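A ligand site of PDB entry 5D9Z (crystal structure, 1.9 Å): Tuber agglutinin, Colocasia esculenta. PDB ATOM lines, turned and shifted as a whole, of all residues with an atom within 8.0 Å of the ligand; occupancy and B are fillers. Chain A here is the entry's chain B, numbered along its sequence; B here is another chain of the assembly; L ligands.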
ATOM      1  N   ASN A   1     -11.108 -37.717   8.573  1.00  0.00           N
ATOM      2  CA  ASN A   1     -11.372 -36.369   9.025  1.00  0.00           C
ATOM      3  C   ASN A   1     -10.084 -35.627   9.308  1.00  0.00           C
ATOM      4  O   ASN A   1      -8.982 -36.177   9.165  1.00  0.00           O
ATOM      5  CB  ASN A   1     -12.245 -36.381  10.279  1.00  0.00           C
ATOM      6  CG  ASN A   1     -13.538 -37.134  10.076  1.00  0.00           C
ATOM      7  OD1 ASN A   1     -13.736 -37.853   9.091  1.00  0.00           O
ATOM      8  ND2 ASN A   1     -14.446 -36.957  11.022  1.00  0.00           N
ATOM      9  N   ILE A   2     -10.238 -34.366   9.730  1.00  0.00           N
ATOM     10  CA  ILE A   2      -9.121 -33.473  10.009  1.00  0.00           C
ATOM     11  C   ILE A   2      -9.035 -33.217  11.498  1.00  0.00           C
ATOM     12  O   ILE A   2     -10.032 -32.891  12.139  1.00  0.00           O
ATOM     13  CB  ILE A   2      -9.322 -32.121   9.321  1.00  0.00           C
ATOM     14  CG1 ILE A   2      -9.532 -32.332   7.834  1.00  0.00           C
ATOM     15  CG2 ILE A   2      -8.154 -31.188   9.537  1.00  0.00           C
ATOM     16  CD1 ILE A   2      -9.818 -31.040   7.116  1.00  0.00           C
ATOM     17  N   PHE A  10     -11.210 -25.768   8.901  1.00  0.00           N
ATOM     18  CA  PHE A  10     -10.962 -25.919   7.480  1.00  0.00           C
ATOM     19  C   PHE A  10     -12.174 -26.481   6.835  1.00  0.00           C
ATOM     20  O   PHE A  10     -12.941 -27.190   7.476  1.00  0.00           O
ATOM     21  CB  PHE A  10      -9.833 -26.884   7.236  1.00  0.00           C
ATOM     22  CG  PHE A  10      -8.523 -26.450   7.805  1.00  0.00           C
ATOM     23  CD1 PHE A  10      -8.197 -26.757   9.102  1.00  0.00           C
ATOM     24  CD2 PHE A  10      -7.602 -25.760   7.040  1.00  0.00           C
ATOM     25  CE1 PHE A  10      -6.959 -26.376   9.644  1.00  0.00           C
ATOM     26  CE2 PHE A  10      -6.372 -25.377   7.576  1.00  0.00           C
ATOM     27  CZ  PHE A  10      -6.051 -25.692   8.877  1.00  0.00           C
ATOM     28  N   SER A  11     -12.342 -26.182   5.555  1.00  0.00           N
ATOM     29  CA  SER A  11     -13.407 -26.735   4.756  1.00  0.00           C
ATOM     30  C   SER A  11     -13.532 -28.201   5.036  1.00  0.00           C
ATOM     31  O   SER A  11     -12.542 -28.938   4.887  1.00  0.00           O
ATOM     32  CB  SER A  11     -13.094 -26.551   3.286  1.00  0.00           C
ATOM     33  OG  SER A  11     -13.080 -25.193   2.975  1.00  0.00           O
ATOM     34  N   GLY A  12     -14.721 -28.625   5.460  1.00  0.00           N
ATOM     35  CA  GLY A  12     -14.996 -30.014   5.799  1.00  0.00           C
ATOM     36  C   GLY A  12     -15.442 -30.239   7.239  1.00  0.00           C
ATOM     37  O   GLY A  12     -16.427 -30.908   7.489  1.00  0.00           O
ATOM     38  N   GLN A  13     -14.710 -29.666   8.182  1.00  0.00           N
ATOM     39  CA  GLN A  13     -15.032 -29.835   9.590  1.00  0.00           C
ATOM     40  C   GLN A  13     -16.358 -29.220   9.906  1.00  0.00           C
ATOM     41  O   GLN A  13     -16.865 -28.382   9.175  1.00  0.00           O
ATOM     42  CB  GLN A  13     -13.944 -29.200  10.403  1.00  0.00           C
ATOM     43  CG  GLN A  13     -12.613 -29.519   9.814  1.00  0.00           C
ATOM     44  CD  GLN A  13     -11.514 -29.044  10.688  1.00  0.00           C
ATOM     45  OE1 GLN A  13     -11.424 -27.848  10.993  1.00  0.00           O
ATOM     46  NE2 GLN A  13     -10.675 -29.957  11.131  1.00  0.00           N
ATOM     47  N   ARG A  59     -20.742 -25.546   9.218  1.00  0.00           N
ATOM     48  CA  ARG A  59     -19.786 -26.128   8.278  1.00  0.00           C
ATOM     49  C   ARG A  59     -19.409 -25.220   7.118  1.00  0.00           C
ATOM     50  O   ARG A  59     -20.256 -24.797   6.310  1.00  0.00           O
ATOM     51  CB  ARG A  59     -20.309 -27.441   7.736  1.00  0.00           C
ATOM     52  CG  ARG A  59     -19.529 -27.941   6.556  1.00  0.00           C
ATOM     53  CD  ARG A  59     -20.258 -29.113   5.939  1.00  0.00           C
ATOM     54  NE  ARG A  59     -19.342 -30.003   5.246  1.00  0.00           N
ATOM     55  CZ  ARG A  59     -19.098 -29.940   3.944  1.00  0.00           C
ATOM     56  NH1 ARG A  59     -19.704 -29.022   3.214  1.00  0.00           N
ATOM     57  NH2 ARG A  59     -18.252 -30.789   3.378  1.00  0.00           N
ATOM     58  N   ASN A  61     -17.786 -24.826   3.679  1.00  0.00           N
ATOM     59  CA  ASN A  61     -17.641 -25.778   2.581  1.00  0.00           C
ATOM     60  C   ASN A  61     -16.374 -25.543   1.785  1.00  0.00           C
ATOM     61  O   ASN A  61     -15.453 -24.932   2.283  1.00  0.00           O
ATOM     62  CB  ASN A  61     -18.837 -25.765   1.642  1.00  0.00           C
ATOM     63  CG  ASN A  61     -19.007 -24.442   0.939  1.00  0.00           C
ATOM     64  OD1 ASN A  61     -18.039 -23.722   0.663  1.00  0.00           O
ATOM     65  ND2 ASN A  61     -20.244 -24.114   0.637  1.00  0.00           N
ATOM     66  N   HIS A  62     -16.365 -25.998   0.531  1.00  0.00           N
ATOM     67  CA  HIS A  62     -15.182 -25.833  -0.313  1.00  0.00           C
ATOM     68  C   HIS A  62     -15.419 -24.787  -1.371  1.00  0.00           C
ATOM     69  O   HIS A  62     -14.670 -24.708  -2.332  1.00  0.00           O
ATOM     70  CB  HIS A  62     -14.810 -27.135  -1.034  1.00  0.00           C
ATOM     71  CG  HIS A  62     -14.188 -28.161  -0.154  1.00  0.00           C
ATOM     72  ND1 HIS A  62     -14.920 -28.955   0.687  1.00  0.00           N
ATOM     73  CD2 HIS A  62     -12.900 -28.544  -0.007  1.00  0.00           C
ATOM     74  CE1 HIS A  62     -14.112 -29.775   1.337  1.00  0.00           C
ATOM     75  NE2 HIS A  62     -12.874 -29.541   0.936  1.00  0.00           N
ATOM     76  N   GLY A  86     -12.248 -24.636  -3.964  1.00  0.00           N
ATOM     77  CA  GLY A  86     -10.995 -25.140  -3.437  1.00  0.00           C
ATOM     78  C   GLY A  86     -11.035 -25.267  -1.923  1.00  0.00           C
ATOM     79  O   GLY A  86     -12.113 -25.328  -1.341  1.00  0.00           O
ATOM     80  N   ASP A  87      -9.865 -25.288  -1.287  1.00  0.00           N
ATOM     81  CA  ASP A  87      -9.799 -25.457   0.154  1.00  0.00           C
ATOM     82  C   ASP A  87      -9.860 -24.118   0.931  1.00  0.00           C
ATOM     83  O   ASP A  87      -9.072 -23.214   0.704  1.00  0.00           O
ATOM     84  CB  ASP A  87      -8.529 -26.240   0.526  1.00  0.00           C
ATOM     85  CG  ASP A  87      -8.600 -27.717   0.143  1.00  0.00           C
ATOM     86  OD1 ASP A  87      -9.708 -28.267  -0.023  1.00  0.00           O
ATOM     87  OD2 ASP A  87      -7.528 -28.348   0.009  1.00  0.00           O
ATOM     88  N   TYR A  88     -10.803 -24.015   1.862  1.00  0.00           N
ATOM     89  CA  TYR A  88     -10.966 -22.800   2.641  1.00  0.00           C
ATOM     90  C   TYR A  88     -10.708 -23.078   4.121  1.00  0.00           C
ATOM     91  O   TYR A  88     -10.648 -24.246   4.530  1.00  0.00           O
ATOM     92  CB  TYR A  88     -12.363 -22.223   2.447  1.00  0.00           C
ATOM     93  CG  TYR A  88     -12.542 -21.587   1.097  1.00  0.00           C
ATOM     94  CD1 TYR A  88     -12.628 -22.360  -0.036  1.00  0.00           C
ATOM     95  CD2 TYR A  88     -12.618 -20.222   0.974  1.00  0.00           C
ATOM     96  CE1 TYR A  88     -12.766 -21.785  -1.263  1.00  0.00           C
ATOM     97  CE2 TYR A  88     -12.755 -19.632  -0.251  1.00  0.00           C
ATOM     98  CZ  TYR A  88     -12.832 -20.418  -1.367  1.00  0.00           C
ATOM     99  OH  TYR A  88     -12.978 -19.840  -2.601  1.00  0.00           O
ATOM    100  N   ALA A 104      -6.925 -21.956  -1.442  1.00  0.00           N
ATOM    101  CA  ALA A 104      -5.515 -22.219  -1.195  1.00  0.00           C
ATOM    102  C   ALA A 104      -4.655 -22.049  -2.462  1.00  0.00           C
ATOM    103  O   ALA A 104      -4.921 -22.666  -3.492  1.00  0.00           O
ATOM    104  CB  ALA A 104      -5.344 -23.596  -0.605  1.00  0.00           C
ATOM    105  N   GLU A 107       1.318 -24.397  -1.250  1.00  0.00           N
ATOM    106  CA  GLU A 107       1.577 -25.351  -0.158  1.00  0.00           C
ATOM    107  C   GLU A 107       3.014 -25.897  -0.142  1.00  0.00           C
ATOM    108  O   GLU A 107       3.711 -25.866  -1.168  1.00  0.00           O
ATOM    109  CB  GLU A 107       0.582 -26.513  -0.226  1.00  0.00           C
ATOM    110  CG  GLU A 107       0.828 -27.449  -1.422  1.00  0.00           C
ATOM    111  CD  GLU A 107      -0.302 -28.450  -1.673  1.00  0.00           C
ATOM    112  OE1 GLU A 107      -0.157 -29.300  -2.582  1.00  0.00           O
ATOM    113  OE2 GLU A 107      -1.329 -28.370  -0.965  1.00  0.00           O
ATOM    114  N   PRO A 110       1.417 -31.740  -0.952  1.00  0.00           N
ATOM    115  CA  PRO A 110      -0.021 -32.045  -1.126  1.00  0.00           C
ATOM    116  C   PRO A 110      -0.653 -32.979  -0.085  1.00  0.00           C
ATOM    117  O   PRO A 110       0.036 -33.841   0.470  1.00  0.00           O
ATOM    118  CB  PRO A 110      -0.055 -32.717  -2.493  1.00  0.00           C
ATOM    119  CG  PRO A 110       1.232 -33.478  -2.542  1.00  0.00           C
ATOM    120  CD  PRO A 110       2.246 -32.595  -1.831  1.00  0.00           C
ATOM    121  N   GLN A 111      -1.955 -32.821   0.121  1.00  0.00           N
ATOM    122  CA  GLN A 111      -2.713 -33.491   1.188  1.00  0.00           C
ATOM    123  C   GLN A 111      -2.407 -34.986   1.363  1.00  0.00           C
ATOM    124  O   GLN A 111      -1.684 -35.384   2.293  1.00  0.00           O
ATOM    125  CB  GLN A 111      -4.216 -33.218   1.022  1.00  0.00           C
ATOM    126  CG  GLN A 111      -5.132 -34.083   1.915  1.00  0.00           C
ATOM    127  CD  GLN A 111      -4.888 -33.910   3.427  1.00  0.00           C
ATOM    128  OE1 GLN A 111      -5.430 -32.985   4.039  1.00  0.00           O
ATOM    129  NE2 GLN A 111      -4.082 -34.805   4.024  1.00  0.00           N
ATOM    130  N   ALA A 112      -2.955 -35.821   0.485  1.00  0.00           N
ATOM    131  CA  ALA A 112      -2.768 -37.274   0.607  1.00  0.00           C
ATOM    132  C   ALA A 112      -1.443 -37.699  -0.024  1.00  0.00           C
ATOM    133  O   ALA A 112      -0.829 -36.944  -0.786  1.00  0.00           O
ATOM    134  CB  ALA A 112      -3.938 -38.025  -0.021  1.00  0.00           C
ATOM    135  N   HIS B  88      -1.383 -26.150   8.832  1.00  0.00           N
ATOM    136  CA  HIS B  88      -2.334 -27.240   8.815  1.00  0.00           C
ATOM    137  C   HIS B  88      -1.851 -28.370   9.716  1.00  0.00           C
ATOM    138  O   HIS B  88      -0.646 -28.657   9.756  1.00  0.00           O
ATOM    139  CB  HIS B  88      -2.471 -27.749   7.401  1.00  0.00           C
ATOM    140  CG  HIS B  88      -3.639 -28.645   7.211  1.00  0.00           C
ATOM    141  ND1 HIS B  88      -3.670 -29.948   7.669  1.00  0.00           N
ATOM    142  CD2 HIS B  88      -4.831 -28.434   6.614  1.00  0.00           C
ATOM    143  CE1 HIS B  88      -4.821 -30.502   7.348  1.00  0.00           C
ATOM    144  NE2 HIS B  88      -5.548 -29.603   6.707  1.00  0.00           N
ATOM    145  N   ASP B  90      -2.002 -31.469   9.322  1.00  0.00           N
ATOM    146  CA  ASP B  90      -1.382 -32.613   8.659  1.00  0.00           C
ATOM    147  C   ASP B  90       0.122 -32.395   8.524  1.00  0.00           C
ATOM    148  O   ASP B  90       0.870 -33.326   8.220  1.00  0.00           O
ATOM    149  CB  ASP B  90      -2.029 -32.954   7.313  1.00  0.00           C
ATOM    150  CG  ASP B  90      -1.944 -31.819   6.300  1.00  0.00           C
ATOM    151  OD1 ASP B  90      -0.993 -31.004   6.340  1.00  0.00           O
ATOM    152  OD2 ASP B  90      -2.865 -31.725   5.459  1.00  0.00           O
ATOM    153  N   ARG B  92       1.406 -29.430   6.733  1.00  0.00           N
ATOM    154  CA  ARG B  92       1.718 -28.582   5.600  1.00  0.00           C
ATOM    155  C   ARG B  92       1.579 -27.136   5.999  1.00  0.00           C
ATOM    156  O   ARG B  92       0.827 -26.819   6.917  1.00  0.00           O
ATOM    157  CB  ARG B  92       0.809 -28.914   4.422  1.00  0.00           C
ATOM    158  CG  ARG B  92       1.019 -30.326   3.949  1.00  0.00           C
ATOM    159  CD  ARG B  92      -0.054 -30.823   3.037  1.00  0.00           C
ATOM    160  NE  ARG B  92      -1.406 -30.515   3.491  1.00  0.00           N
ATOM    161  CZ  ARG B  92      -2.192 -29.617   2.903  1.00  0.00           C
ATOM    162  NH1 ARG B  92      -1.728 -28.950   1.848  1.00  0.00           N
ATOM    163  NH2 ARG B  92      -3.415 -29.383   3.355  1.00  0.00           N
ATOM    164  N   VAL B  94       0.134 -23.805   4.468  1.00  0.00           N
ATOM    165  CA  VAL B  94      -0.732 -23.393   3.365  1.00  0.00           C
ATOM    166  C   VAL B  94      -1.011 -21.882   3.399  1.00  0.00           C
ATOM    167  O   VAL B  94      -1.323 -21.334   4.472  1.00  0.00           O
ATOM    168  CB  VAL B  94      -2.034 -24.174   3.416  1.00  0.00           C
ATOM    169  CG1 VAL B  94      -2.905 -23.852   2.227  1.00  0.00           C
ATOM    170  CG2 VAL B  94      -1.722 -25.666   3.444  1.00  0.00           C
ATOM    171  N   PHE B  96      -3.552 -19.249   2.474  1.00  0.00           N
ATOM    172  CA  PHE B  96      -4.936 -19.128   2.073  1.00  0.00           C
ATOM    173  C   PHE B  96      -5.187 -17.683   1.786  1.00  0.00           C
ATOM    174  O   PHE B  96      -4.491 -16.816   2.314  1.00  0.00           O
ATOM    175  CB  PHE B  96      -5.880 -19.523   3.210  1.00  0.00           C
ATOM    176  CG  PHE B  96      -5.954 -21.003   3.504  1.00  0.00           C
ATOM    177  CD1 PHE B  96      -6.894 -21.807   2.873  1.00  0.00           C
ATOM    178  CD2 PHE B  96      -5.128 -21.589   4.458  1.00  0.00           C
ATOM    179  CE1 PHE B  96      -6.974 -23.147   3.156  1.00  0.00           C
ATOM    180  CE2 PHE B  96      -5.210 -22.932   4.758  1.00  0.00           C
ATOM    181  CZ  PHE B  96      -6.136 -23.703   4.106  1.00  0.00           C
HETATM  182  C1  LIG L   1      -7.937 -31.581   2.341  1.00  0.00           C
HETATM  183  C2  LIG L   1      -9.455 -31.633   2.231  1.00  0.00           C
HETATM  184  C3  LIG L   1      -9.798 -32.386   0.996  1.00  0.00           C
HETATM  185  C4  LIG L   1      -9.165 -31.668  -0.177  1.00  0.00           C
HETATM  186  C5  LIG L   1      -7.650 -31.725   0.027  1.00  0.00           C
HETATM  187  C6  LIG L   1      -6.837 -31.195  -1.148  1.00  0.00           C
HETATM  188  O1  LIG L   1      -7.549 -30.870   3.494  1.00  0.00           O
HETATM  189  O2  LIG L   1     -10.029 -30.362   2.047  1.00  0.00           O
HETATM  190  O3  LIG L   1     -11.194 -32.337   0.917  1.00  0.00           O
HETATM  191  O4  LIG L   1      -9.514 -32.321  -1.373  1.00  0.00           O
HETATM  192  O5  LIG L   1      -7.372 -30.988   1.192  1.00  0.00           O
HETATM  193  O6  LIG L   1      -6.869 -32.091  -2.243  1.00  0.00           O
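An oxygen (O2) of the ligand lies within hydrogen-bond range of the side-chain carboxylate (OD1) of Asp 87, 3.0 Å away.
A ring nitrogen (NE2) of His 62 sits at hydrogen-bond distance from an oxygen (O2) of the ligand.
An oxygen (O1) of the ligand is in hydrogen-bond range of the side-chain amide oxygen of Gln 111.
The backbone NH of Ala 104 is in hydrogen-bond range of the backbone carbonyl oxygen of Asp 87, at 3.3 Å.
OD2 of Asp 90 of chain B sits close to OE1 of Gln 111 (3.2 Å).
O of His 62 sits at hydrogen-bond distance from N of Gly 86 (2.9 Å).
ND1 of His 88 of chain B lies within hydrogen-bond range of N of Asp 90 of chain B, at 2.8 Å.
Merely in contact with the ligand: His 88 of chain B (3.99 Å).
Of the 22 residues printed, 4 come within 4 Å of the ligand.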
